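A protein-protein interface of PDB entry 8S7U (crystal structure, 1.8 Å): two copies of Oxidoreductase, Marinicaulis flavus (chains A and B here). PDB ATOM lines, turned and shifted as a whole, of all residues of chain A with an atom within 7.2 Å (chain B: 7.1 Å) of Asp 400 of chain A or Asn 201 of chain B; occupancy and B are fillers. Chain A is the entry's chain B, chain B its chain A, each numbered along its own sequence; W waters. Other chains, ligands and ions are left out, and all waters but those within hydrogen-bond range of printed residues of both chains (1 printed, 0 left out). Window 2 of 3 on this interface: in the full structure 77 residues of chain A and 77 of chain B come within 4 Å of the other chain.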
ATOM      1  N   GLU A 254      -7.113  23.275   8.642  1.00  0.00           N
ATOM      2  CA  GLU A 254      -5.747  23.495   8.092  1.00  0.00           C
ATOM      3  C   GLU A 254      -4.733  22.668   8.865  1.00  0.00           C
ATOM      4  O   GLU A 254      -4.011  21.832   8.270  1.00  0.00           O
ATOM      5  CB  GLU A 254      -5.368  24.984   8.113  1.00  0.00           C
ATOM      6  CG  GLU A 254      -4.017  25.229   7.487  1.00  0.00           C
ATOM      7  CD  GLU A 254      -3.714  26.693   7.216  1.00  0.00           C
ATOM      8  OE1 GLU A 254      -4.575  27.527   7.383  1.00  0.00           O
ATOM      9  OE2 GLU A 254      -2.633  26.960   6.759  1.00  0.00           O
ATOM     10  N   THR A 257      -5.437  18.732   8.694  1.00  0.00           N
ATOM     11  CA  THR A 257      -4.986  18.107   7.418  1.00  0.00           C
ATOM     12  C   THR A 257      -3.466  17.939   7.421  1.00  0.00           C
ATOM     13  O   THR A 257      -2.954  16.873   6.959  1.00  0.00           O
ATOM     14  CB  THR A 257      -5.542  18.896   6.234  1.00  0.00           C
ATOM     15  OG1 THR A 257      -6.969  18.971   6.360  1.00  0.00           O
ATOM     16  CG2 THR A 257      -5.225  18.204   4.930  1.00  0.00           C
ATOM     17  N   GLU A 258      -2.719  18.921   7.924  1.00  0.00           N
ATOM     18  CA  GLU A 258      -1.250  18.793   7.984  1.00  0.00           C
ATOM     19  C   GLU A 258      -0.868  17.564   8.843  1.00  0.00           C
ATOM     20  O   GLU A 258       0.089  16.811   8.486  1.00  0.00           O
ATOM     21  CB  GLU A 258      -0.654  20.094   8.561  1.00  0.00           C
ATOM     22  CG  GLU A 258      -0.656  21.268   7.593  1.00  0.00           C
ATOM     23  CD  GLU A 258       0.148  20.966   6.340  1.00  0.00           C
ATOM     24  OE1 GLU A 258       1.361  20.756   6.521  1.00  0.00           O
ATOM     25  OE2 GLU A 258      -0.462  20.839   5.196  1.00  0.00           O
ATOM     26  N   VAL A 393     -11.021  17.033  -5.985  1.00  0.00           N
ATOM     27  CA  VAL A 393      -9.929  16.296  -5.295  1.00  0.00           C
ATOM     28  C   VAL A 393      -8.997  17.338  -4.677  1.00  0.00           C
ATOM     29  O   VAL A 393      -8.810  18.391  -5.293  1.00  0.00           O
ATOM     30  CB  VAL A 393      -9.150  15.397  -6.277  1.00  0.00           C
ATOM     31  CG1 VAL A 393      -7.968  14.704  -5.620  1.00  0.00           C
ATOM     32  CG2 VAL A 393     -10.066  14.388  -6.951  1.00  0.00           C
ATOM     33  N   SER A 394      -8.427  17.033  -3.521  1.00  0.00           N
ATOM     34  CA  SER A 394      -7.440  17.948  -2.906  1.00  0.00           C
ATOM     35  C   SER A 394      -6.216  17.179  -2.435  1.00  0.00           C
ATOM     36  O   SER A 394      -6.346  16.010  -2.071  1.00  0.00           O
ATOM     37  CB  SER A 394      -8.015  18.699  -1.725  1.00  0.00           C
ATOM     38  OG  SER A 394      -7.010  19.386  -1.004  1.00  0.00           O
ATOM     39  N   PRO A 395      -5.029  17.801  -2.455  1.00  0.00           N
ATOM     40  CA  PRO A 395      -3.895  17.187  -1.814  1.00  0.00           C
ATOM     41  C   PRO A 395      -4.221  17.090  -0.313  1.00  0.00           C
ATOM     42  O   PRO A 395      -5.076  17.805   0.146  1.00  0.00           O
ATOM     43  CB  PRO A 395      -2.788  18.226  -2.017  1.00  0.00           C
ATOM     44  CG  PRO A 395      -3.214  19.032  -3.218  1.00  0.00           C
ATOM     45  CD  PRO A 395      -4.724  19.044  -3.157  1.00  0.00           C
ATOM     46  N   ILE A 396      -3.547  16.196   0.406  1.00  0.00           N
ATOM     47  CA  ILE A 396      -3.710  16.154   1.886  1.00  0.00           C
ATOM     48  C   ILE A 396      -2.816  17.261   2.461  1.00  0.00           C
ATOM     49  O   ILE A 396      -1.778  16.943   3.036  1.00  0.00           O
ATOM     50  CB  ILE A 396      -3.406  14.763   2.479  1.00  0.00           C
ATOM     51  CG1 ILE A 396      -4.066  13.639   1.679  1.00  0.00           C
ATOM     52  CG2 ILE A 396      -3.802  14.715   3.945  1.00  0.00           C
ATOM     53  CD1 ILE A 396      -3.806  12.264   2.239  1.00  0.00           C
ATOM     54  N   THR A 397      -3.205  18.517   2.239  1.00  0.00           N
ATOM     55  CA  THR A 397      -2.458  19.676   2.782  1.00  0.00           C
ATOM     56  C   THR A 397      -3.468  20.681   3.335  1.00  0.00           C
ATOM     57  O   THR A 397      -4.520  20.855   2.720  1.00  0.00           O
ATOM     58  CB  THR A 397      -1.576  20.349   1.724  1.00  0.00           C
ATOM     59  OG1 THR A 397      -2.425  21.218   0.981  1.00  0.00           O
ATOM     60  CG2 THR A 397      -0.886  19.365   0.810  1.00  0.00           C
ATOM     61  N   GLY A 398      -3.138  21.328   4.444  1.00  0.00           N
ATOM     62  CA  GLY A 398      -4.111  22.238   5.070  1.00  0.00           C
ATOM     63  C   GLY A 398      -4.484  23.384   4.153  1.00  0.00           C
ATOM     64  O   GLY A 398      -5.648  23.734   4.097  1.00  0.00           O
ATOM     65  N   LYS A 399      -3.495  23.958   3.484  1.00  0.00           N
ATOM     66  CA  LYS A 399      -3.749  25.125   2.604  1.00  0.00           C
ATOM     67  C   LYS A 399      -4.850  24.791   1.603  1.00  0.00           C
ATOM     68  O   LYS A 399      -5.744  25.598   1.421  1.00  0.00           O
ATOM     69  CB  LYS A 399      -2.469  25.478   1.854  1.00  0.00           C
ATOM     70  CG  LYS A 399      -2.579  26.645   0.885  1.00  0.00           C
ATOM     71  CD  LYS A 399      -1.284  26.921   0.152  1.00  0.00           C
ATOM     72  CE  LYS A 399      -1.338  28.169  -0.703  1.00  0.00           C
ATOM     73  NZ  LYS A 399      -1.338  29.396   0.127  1.00  0.00           N
ATOM     74  N   ASP A 400      -4.742  23.631   0.966  1.00  0.00           N
ATOM     75  CA  ASP A 400      -5.729  23.241  -0.070  1.00  0.00           C
ATOM     76  C   ASP A 400      -7.088  22.949   0.580  1.00  0.00           C
ATOM     77  O   ASP A 400      -8.096  23.415   0.072  1.00  0.00           O
ATOM     78  CB  ASP A 400      -5.198  22.055  -0.872  1.00  0.00           C
ATOM     79  CG  ASP A 400      -3.965  22.410  -1.684  1.00  0.00           C
ATOM     80  OD1 ASP A 400      -4.103  23.160  -2.656  1.00  0.00           O
ATOM     81  OD2 ASP A 400      -2.884  21.941  -1.324  1.00  0.00           O
ATOM     82  N   ALA A 401      -7.077  22.202   1.677  1.00  0.00           N
ATOM     83  CA  ALA A 401      -8.337  21.846   2.372  1.00  0.00           C
ATOM     84  C   ALA A 401      -9.097  23.108   2.811  1.00  0.00           C
ATOM     85  O   ALA A 401     -10.278  23.213   2.523  1.00  0.00           O
ATOM     86  CB  ALA A 401      -8.024  20.949   3.536  1.00  0.00           C
ATOM     87  N   ILE A 402      -8.413  24.026   3.486  1.00  0.00           N
ATOM     88  CA  ILE A 402      -9.089  25.259   3.987  1.00  0.00           C
ATOM     89  C   ILE A 402      -9.508  26.138   2.799  1.00  0.00           C
ATOM     90  O   ILE A 402     -10.567  26.751   2.867  1.00  0.00           O
ATOM     91  CB  ILE A 402      -8.228  26.022   5.016  1.00  0.00           C
ATOM     92  CG1 ILE A 402      -9.097  26.988   5.826  1.00  0.00           C
ATOM     93  CG2 ILE A 402      -7.053  26.727   4.362  1.00  0.00           C
ATOM     94  CD1 ILE A 402      -8.610  27.236   7.226  1.00  0.00           C
ATOM     95  N   LYS A 403      -8.701  26.157   1.737  1.00  0.00           N
ATOM     96  CA  LYS A 403      -9.059  26.959   0.539  1.00  0.00           C
ATOM     97  C   LYS A 403     -10.363  26.417  -0.054  1.00  0.00           C
ATOM     98  O   LYS A 403     -11.281  27.193  -0.278  1.00  0.00           O
ATOM     99  CB  LYS A 403      -7.934  26.942  -0.498  1.00  0.00           C
ATOM    100  CG  LYS A 403      -8.249  27.609  -1.827  1.00  0.00           C
ATOM    101  CD  LYS A 403      -8.708  29.042  -1.682  1.00  0.00           C
ATOM    102  CE  LYS A 403      -8.781  29.783  -3.000  1.00  0.00           C
ATOM    103  NZ  LYS A 403      -8.929  31.247  -2.809  1.00  0.00           N
ATOM    104  N   GLN A 404     -10.402  25.115  -0.310  1.00  0.00           N
ATOM    105  CA  GLN A 404     -11.610  24.510  -0.927  1.00  0.00           C
ATOM    106  C   GLN A 404     -12.810  24.700   0.011  1.00  0.00           C
ATOM    107  O   GLN A 404     -13.874  25.069  -0.468  1.00  0.00           O
ATOM    108  CB  GLN A 404     -11.363  23.038  -1.256  1.00  0.00           C
ATOM    109  CG  GLN A 404     -10.356  22.800  -2.369  1.00  0.00           C
ATOM    110  CD  GLN A 404     -10.451  21.399  -2.923  1.00  0.00           C
ATOM    111  OE1 GLN A 404     -11.324  20.622  -2.550  1.00  0.00           O
ATOM    112  NE2 GLN A 404      -9.545  21.059  -3.823  1.00  0.00           N
ATOM    113  N   TYR A 405     -12.611  24.466   1.306  1.00  0.00           N
ATOM    114  CA  TYR A 405     -13.708  24.685   2.280  1.00  0.00           C
ATOM    115  C   TYR A 405     -14.262  26.104   2.122  1.00  0.00           C
ATOM    116  O   TYR A 405     -15.462  26.274   1.980  1.00  0.00           O
ATOM    117  CB  TYR A 405     -13.226  24.502   3.717  1.00  0.00           C
ATOM    118  CG  TYR A 405     -14.193  25.021   4.747  1.00  0.00           C
ATOM    119  CD1 TYR A 405     -15.464  24.488   4.851  1.00  0.00           C
ATOM    120  CD2 TYR A 405     -13.850  26.055   5.600  1.00  0.00           C
ATOM    121  CE1 TYR A 405     -16.369  24.958   5.784  1.00  0.00           C
ATOM    122  CE2 TYR A 405     -14.743  26.539   6.539  1.00  0.00           C
ATOM    123  CZ  TYR A 405     -16.006  25.985   6.634  1.00  0.00           C
ATOM    124  OH  TYR A 405     -16.908  26.446   7.550  1.00  0.00           O
ATOM    125  N   ASN A 406     -13.364  27.080   2.154  1.00  0.00           N
ATOM    126  CA  ASN A 406     -13.781  28.503   2.074  1.00  0.00           C
ATOM    127  C   ASN A 406     -14.506  28.772   0.755  1.00  0.00           C
ATOM    128  O   ASN A 406     -15.549  29.408   0.799  1.00  0.00           O
ATOM    129  CB  ASN A 406     -12.572  29.419   2.267  1.00  0.00           C
ATOM    130  CG  ASN A 406     -12.107  29.488   3.706  1.00  0.00           C
ATOM    131  OD1 ASN A 406     -12.914  29.423   4.627  1.00  0.00           O
ATOM    132  ND2 ASN A 406     -10.808  29.631   3.910  1.00  0.00           N
ATOM    133  N   MET A 407     -13.950  28.302  -0.361  1.00  0.00           N
ATOM    134  CA  MET A 407     -14.534  28.577  -1.700  1.00  0.00           C
ATOM    135  C   MET A 407     -15.919  27.933  -1.832  1.00  0.00           C
ATOM    136  O   MET A 407     -16.820  28.576  -2.356  1.00  0.00           O
ATOM    137  CB  MET A 407     -13.645  27.984  -2.794  1.00  0.00           C
ATOM    138  CG  MET A 407     -12.256  28.560  -2.887  1.00  0.00           C
ATOM    139  SD  MET A 407     -11.293  27.636  -4.115  1.00  0.00           S
ATOM    140  CE  MET A 407     -12.195  28.026  -5.611  1.00  0.00           C
ATOM    141  N   LEU A 430      -7.335  13.780  -0.870  1.00  0.00           N
ATOM    142  CA  LEU A 430      -8.638  13.898  -0.186  1.00  0.00           C
ATOM    143  C   LEU A 430      -9.725  14.022  -1.252  1.00  0.00           C
ATOM    144  O   LEU A 430      -9.552  14.825  -2.170  1.00  0.00           O
ATOM    145  CB  LEU A 430      -8.681  15.151   0.685  1.00  0.00           C
ATOM    146  CG  LEU A 430      -7.698  15.209   1.850  1.00  0.00           C
ATOM    147  CD1 LEU A 430      -7.806  16.549   2.557  1.00  0.00           C
ATOM    148  CD2 LEU A 430      -7.954  14.073   2.825  1.00  0.00           C
ATOM    149  N   HIS A 432     -12.982  15.610  -1.749  1.00  0.00           N
ATOM    150  CA  HIS A 432     -13.819  16.634  -1.075  1.00  0.00           C
ATOM    151  C   HIS A 432     -15.223  16.596  -1.677  1.00  0.00           C
ATOM    152  O   HIS A 432     -15.484  17.277  -2.659  1.00  0.00           O
ATOM    153  CB  HIS A 432     -13.174  18.017  -1.172  1.00  0.00           C
ATOM    154  CG  HIS A 432     -13.928  19.101  -0.490  1.00  0.00           C
ATOM    155  ND1 HIS A 432     -13.640  20.431  -0.689  1.00  0.00           N
ATOM    156  CD2 HIS A 432     -14.937  19.067   0.384  1.00  0.00           C
ATOM    157  CE1 HIS A 432     -14.462  21.167   0.041  1.00  0.00           C
ATOM    158  NE2 HIS A 432     -15.259  20.359   0.695  1.00  0.00           N
ATOM    159  N   GLU A 463      -8.605  27.324  -9.824  1.00  0.00           N
ATOM    160  CA  GLU A 463      -7.594  27.081  -8.768  1.00  0.00           C
ATOM    161  C   GLU A 463      -6.876  25.746  -9.010  1.00  0.00           C
ATOM    162  O   GLU A 463      -6.163  25.305  -8.121  1.00  0.00           O
ATOM    163  CB  GLU A 463      -8.255  27.110  -7.394  1.00  0.00           C
ATOM    164  CG  GLU A 463      -8.614  28.500  -6.924  1.00  0.00           C
ATOM    165  CD  GLU A 463      -7.420  29.269  -6.392  1.00  0.00           C
ATOM    166  OE1 GLU A 463      -6.525  28.637  -5.810  1.00  0.00           O
ATOM    167  OE2 GLU A 463      -7.390  30.489  -6.569  1.00  0.00           O
ATOM    168  N   GLY A 464      -7.067  25.136 -10.180  1.00  0.00           N
ATOM    169  CA  GLY A 464      -6.334  23.899 -10.502  1.00  0.00           C
ATOM    170  C   GLY A 464      -6.925  22.680  -9.827  1.00  0.00           C
ATOM    171  O   GLY A 464      -6.203  21.708  -9.643  1.00  0.00           O
ATOM    172  N   TYR A 465      -8.213  22.750  -9.499  1.00  0.00           N
ATOM    173  CA  TYR A 465      -8.900  21.617  -8.834  1.00  0.00           C
ATOM    174  C   TYR A 465      -9.916  20.970  -9.781  1.00  0.00           C
ATOM    175  O   TYR A 465     -10.732  21.692 -10.363  1.00  0.00           O
ATOM    176  CB  TYR A 465      -9.587  22.076  -7.546  1.00  0.00           C
ATOM    177  CG  TYR A 465      -8.685  22.653  -6.486  1.00  0.00           C
ATOM    178  CD1 TYR A 465      -7.482  22.055  -6.153  1.00  0.00           C
ATOM    179  CD2 TYR A 465      -9.056  23.791  -5.791  1.00  0.00           C
ATOM    180  CE1 TYR A 465      -6.667  22.579  -5.164  1.00  0.00           C
ATOM    181  CE2 TYR A 465      -8.251  24.330  -4.805  1.00  0.00           C
ATOM    182  CZ  TYR A 465      -7.051  23.723  -4.490  1.00  0.00           C
ATOM    183  OH  TYR A 465      -6.265  24.268  -3.510  1.00  0.00           O
ATOM    184  N   PHE B 119       4.688  13.707   0.709  1.00  0.00           N
ATOM    185  CA  PHE B 119       3.656  12.834   0.094  1.00  0.00           C
ATOM    186  C   PHE B 119       4.215  11.491  -0.334  1.00  0.00           C
ATOM    187  O   PHE B 119       3.437  10.620  -0.758  1.00  0.00           O
ATOM    188  CB  PHE B 119       3.022  13.516  -1.097  1.00  0.00           C
ATOM    189  CG  PHE B 119       2.007  14.500  -0.644  1.00  0.00           C
ATOM    190  CD1 PHE B 119       0.780  14.042  -0.182  1.00  0.00           C
ATOM    191  CD2 PHE B 119       2.251  15.845  -0.724  1.00  0.00           C
ATOM    192  CE1 PHE B 119      -0.206  14.939   0.179  1.00  0.00           C
ATOM    193  CE2 PHE B 119       1.263  16.750  -0.353  1.00  0.00           C
ATOM    194  CZ  PHE B 119       0.085  16.294   0.158  1.00  0.00           C
ATOM    195  N   TYR B 121       6.481  10.401  -2.972  1.00  0.00           N
ATOM    196  CA  TYR B 121       6.433  10.048  -4.394  1.00  0.00           C
ATOM    197  C   TYR B 121       7.652  10.626  -5.102  1.00  0.00           C
ATOM    198  O   TYR B 121       8.331  11.560  -4.577  1.00  0.00           O
ATOM    199  CB  TYR B 121       5.120  10.568  -4.997  1.00  0.00           C
ATOM    200  CG  TYR B 121       5.026  12.040  -5.228  1.00  0.00           C
ATOM    201  CD1 TYR B 121       5.762  12.684  -6.221  1.00  0.00           C
ATOM    202  CD2 TYR B 121       4.177  12.800  -4.454  1.00  0.00           C
ATOM    203  CE1 TYR B 121       5.583  14.028  -6.466  1.00  0.00           C
ATOM    204  CE2 TYR B 121       3.989  14.142  -4.699  1.00  0.00           C
ATOM    205  CZ  TYR B 121       4.708  14.758  -5.700  1.00  0.00           C
ATOM    206  OH  TYR B 121       4.522  16.103  -5.882  1.00  0.00           O
ATOM    207  N   MET B 194      -4.842  13.437 -12.944  1.00  0.00           N
ATOM    208  CA  MET B 194      -4.991  14.862 -12.630  1.00  0.00           C
ATOM    209  C   MET B 194      -3.987  15.692 -13.487  1.00  0.00           C
ATOM    210  O   MET B 194      -4.101  16.917 -13.477  1.00  0.00           O
ATOM    211  CB  MET B 194      -4.709  15.037 -11.142  1.00  0.00           C
ATOM    212  CG  MET B 194      -5.807  14.377 -10.240  1.00  0.00           C
ATOM    213  SD  MET B 194      -7.471  14.735 -10.690  1.00  0.00           S
ATOM    214  CE  MET B 194      -7.692  16.494 -10.430  1.00  0.00           C
ATOM    215  N   MET B 197      -5.450  18.203 -15.868  1.00  0.00           N
ATOM    216  CA  MET B 197      -6.015  19.462 -15.299  1.00  0.00           C
ATOM    217  C   MET B 197      -4.890  20.494 -15.336  1.00  0.00           C
ATOM    218  O   MET B 197      -3.910  20.377 -14.597  1.00  0.00           O
ATOM    219  CB  MET B 197      -6.515  19.229 -13.874  1.00  0.00           C
ATOM    220  CG  MET B 197      -6.761  20.453 -12.980  1.00  0.00           C
ATOM    221  SD  MET B 197      -7.993  21.570 -13.582  1.00  0.00           S
ATOM    222  CE  MET B 197      -9.428  20.503 -13.673  1.00  0.00           C
ATOM    223  N   PRO B 198      -5.025  21.547 -16.167  1.00  0.00           N
ATOM    224  CA  PRO B 198      -4.020  22.625 -16.133  1.00  0.00           C
ATOM    225  C   PRO B 198      -3.944  23.248 -14.729  1.00  0.00           C
ATOM    226  O   PRO B 198      -4.987  23.472 -14.107  1.00  0.00           O
ATOM    227  CB  PRO B 198      -4.522  23.632 -17.144  1.00  0.00           C
ATOM    228  CG  PRO B 198      -5.598  22.881 -17.951  1.00  0.00           C
ATOM    229  CD  PRO B 198      -6.201  21.857 -16.993  1.00  0.00           C
ATOM    230  N   GLY B 199      -2.743  23.446 -14.236  1.00  0.00           N
ATOM    231  CA  GLY B 199      -2.553  24.100 -12.939  1.00  0.00           C
ATOM    232  C   GLY B 199      -2.753  23.145 -11.768  1.00  0.00           C
ATOM    233  O   GLY B 199      -2.841  23.644 -10.639  1.00  0.00           O
ATOM    234  N   ASN B 200      -2.841  21.821 -11.995  1.00  0.00           N
ATOM    235  CA  ASN B 200      -3.118  20.825 -10.918  1.00  0.00           C
ATOM    236  C   ASN B 200      -1.943  20.774  -9.950  1.00  0.00           C
ATOM    237  O   ASN B 200      -0.796  21.150 -10.304  1.00  0.00           O
ATOM    238  CB  ASN B 200      -3.397  19.417 -11.437  1.00  0.00           C
ATOM    239  CG  ASN B 200      -2.137  18.715 -11.851  1.00  0.00           C
ATOM    240  OD1 ASN B 200      -1.463  18.117 -11.047  1.00  0.00           O
ATOM    241  ND2 ASN B 200      -1.715  18.945 -13.084  1.00  0.00           N
ATOM    242  N   ASN B 201      -2.230  20.304  -8.740  1.00  0.00           N
ATOM    243  CA  ASN B 201      -1.201  19.950  -7.753  1.00  0.00           C
ATOM    244  C   ASN B 201      -1.486  18.531  -7.267  1.00  0.00           C
ATOM    245  O   ASN B 201      -1.153  18.263  -6.107  1.00  0.00           O
ATOM    246  CB  ASN B 201      -1.148  20.996  -6.637  1.00  0.00           C
ATOM    247  CG  ASN B 201      -2.432  21.208  -5.865  1.00  0.00           C
ATOM    248  OD1 ASN B 201      -3.492  20.618  -6.141  1.00  0.00           O
ATOM    249  ND2 ASN B 201      -2.338  22.104  -4.887  1.00  0.00           N
ATOM    250  N   THR B 202      -2.039  17.674  -8.137  1.00  0.00           N
ATOM    251  CA  THR B 202      -2.474  16.315  -7.706  1.00  0.00           C
ATOM    252  C   THR B 202      -2.031  15.198  -8.661  1.00  0.00           C
ATOM    253  O   THR B 202      -2.377  14.057  -8.383  1.00  0.00           O
ATOM    254  CB  THR B 202      -3.984  16.323  -7.458  1.00  0.00           C
ATOM    255  OG1 THR B 202      -4.594  16.983  -8.556  1.00  0.00           O
ATOM    256  CG2 THR B 202      -4.353  17.036  -6.164  1.00  0.00           C
ATOM    257  N   TRP B 203      -1.230  15.463  -9.696  1.00  0.00           N
ATOM    258  CA  TRP B 203      -0.832  14.426 -10.669  1.00  0.00           C
ATOM    259  C   TRP B 203      -0.313  13.166  -9.971  1.00  0.00           C
ATOM    260  O   TRP B 203      -0.625  12.055 -10.421  1.00  0.00           O
ATOM    261  CB  TRP B 203       0.243  15.008 -11.634  1.00  0.00           C
ATOM    262  CG  TRP B 203       0.367  14.260 -12.930  1.00  0.00           C
ATOM    263  CD1 TRP B 203      -0.485  13.326 -13.475  1.00  0.00           C
ATOM    264  CD2 TRP B 203       1.457  14.408 -13.855  1.00  0.00           C
ATOM    265  NE1 TRP B 203      -0.018  12.905 -14.693  1.00  0.00           N
ATOM    266  CE2 TRP B 203       1.151  13.588 -14.968  1.00  0.00           C
ATOM    267  CE3 TRP B 203       2.592  15.236 -13.875  1.00  0.00           C
ATOM    268  CZ2 TRP B 203       2.000  13.529 -16.067  1.00  0.00           C
ATOM    269  CZ3 TRP B 203       3.437  15.165 -14.965  1.00  0.00           C
ATOM    270  CH2 TRP B 203       3.132  14.316 -16.038  1.00  0.00           C
ATOM    271  N   GLN B 204       0.557  13.338  -8.979  1.00  0.00           N
ATOM    272  CA  GLN B 204       1.205  12.209  -8.268  1.00  0.00           C
ATOM    273  C   GLN B 204       0.441  11.832  -6.980  1.00  0.00           C
ATOM    274  O   GLN B 204       0.990  11.071  -6.216  1.00  0.00           O
ATOM    275  CB  GLN B 204       2.684  12.551  -7.993  1.00  0.00           C
ATOM    276  CG  GLN B 204       3.551  12.098  -9.135  1.00  0.00           C
ATOM    277  CD  GLN B 204       3.300  12.867 -10.410  1.00  0.00           C
ATOM    278  OE1 GLN B 204       3.601  14.044 -10.491  1.00  0.00           O
ATOM    279  NE2 GLN B 204       2.723  12.211 -11.419  1.00  0.00           N
ATOM    280  N   LEU B 205      -0.742  12.377  -6.757  1.00  0.00           N
ATOM    281  CA  LEU B 205      -1.514  12.165  -5.515  1.00  0.00           C
ATOM    282  C   LEU B 205      -2.769  11.319  -5.793  1.00  0.00           C
ATOM    283  O   LEU B 205      -3.213  10.645  -4.834  1.00  0.00           O
ATOM    284  CB  LEU B 205      -1.883  13.529  -4.912  1.00  0.00           C
ATOM    285  CG  LEU B 205      -0.690  14.424  -4.506  1.00  0.00           C
ATOM    286  CD1 LEU B 205      -1.201  15.598  -3.700  1.00  0.00           C
ATOM    287  CD2 LEU B 205       0.332  13.630  -3.739  1.00  0.00           C
HETATM  288  O   HOH W   1      -5.237  19.863  -8.083  1.00  0.00           O
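OD1 of Asp 400 of chain A is in hydrogen-bond range of ND2 of Asn 201 of chain B (3.0 Å).
O of Met 194 of chain B sits close to ND2 of Asn 200 of chain B (3.2 Å). ND2 of Asn 200 of chain B lies within hydrogen-bond range of O of Met 197 of chain B, at 3.0 Å. OD1 of Asn 200 of chain B sits at hydrogen-bond distance from N of Thr 202 of chain B, at 3.0 Å. OD1 of Asn 200 of chain B lies within hydrogen-bond range of N of Trp 203 of chain B. OD2 of Asp 400 of chain A sits at hydrogen-bond distance from OG1 of Thr 397 of chain A. The side-chain carboxylate (OD1) of Asp 400 of chain A lies within hydrogen-bond range of the side-chain hydroxyl (OH) of Tyr 465 of chain A, at 2.6 Å.
Pro 395 of chain A touches Asn 201 of chain B (CG to OD1, 3.3 Å). Thr 202 of chain B touches Pro 395 of chain A (CG2 to CD, 3.6 Å). Leu 205 of chain B touches Pro 395 of chain A (CD1 to CB, 3.5 Å). Ile 396 of chain A touches Phe 119 of chain B. O of Gly 464 of chain A touches CG of Met 197 of chain B, at 3.6 Å. O of Pro 198 of chain B touches CA of Gly 464 of chain A (3.9 Å). Gly 199 of chain B touches Gly 464 of chain A. Asn 200 of chain B touches Gly 464 of chain A (CA to O, 3.5 Å). Tyr 465 of chain A touches Met 197 of chain B (O to CE, 3.8 Å). Tyr 465 of chain A touches Asn 201 of chain B.
Asp 400 of chain A touches just one residue of chain B: Asn 201 (3.0 Å). Asn 201 of chain B touches three residues of chain A. Printed residues of chain B within 4 Å of Pro 395 of chain A: Asn 201 (3.3 Å), Thr 202 (3.6 Å) and Leu 205 (3.5 Å). Of the printed residues of chain B, Gly 464 of chain A touches Met 197, Pro 198, Gly 199 and Asn 200. Of the printed residues of chain B, Tyr 465 of chain A touches Met 197 (3.8 Å) and Asn 201 (3.9 Å). Printed residues of chain A within 4 Å of Leu 205 of chain B: Pro 395. The nearest residue of chain B that does not touch Asp 400 of chain A is Phe 119 of chain B (6.5 Å). The nearest printed residue of chain A that does not touch Phe 119 of chain B is Pro 395 of chain A (4.1 Å).
Hydrophobic or aromatic side chains of chain A within 4 Å of the printed part of chain B: Pro 395, Ile 396 and Tyr 465. Along chain A the printed residues that touch a printed residue of chain B span positions 395 to 465. Hydrophobic or aromatic side chains of chain B within 4 Å of the printed part of chain A: Phe 119, Met 197 and Leu 205. Along chain B the printed residues that touch a printed residue of chain A span positions 119 to 205.
No position is printed for both chains. Of the 12 pairs that touch across the chains among the printed residues, none has its exchanged pair printed and touching as well.
Water W1 lies within hydrogen-bond range of O of Gly 464 of chain A (2.6 Å), OD1 of Asn 201 of chain B (2.7 Å) and OG1 of Thr 202 of chain B (3.0 Å).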
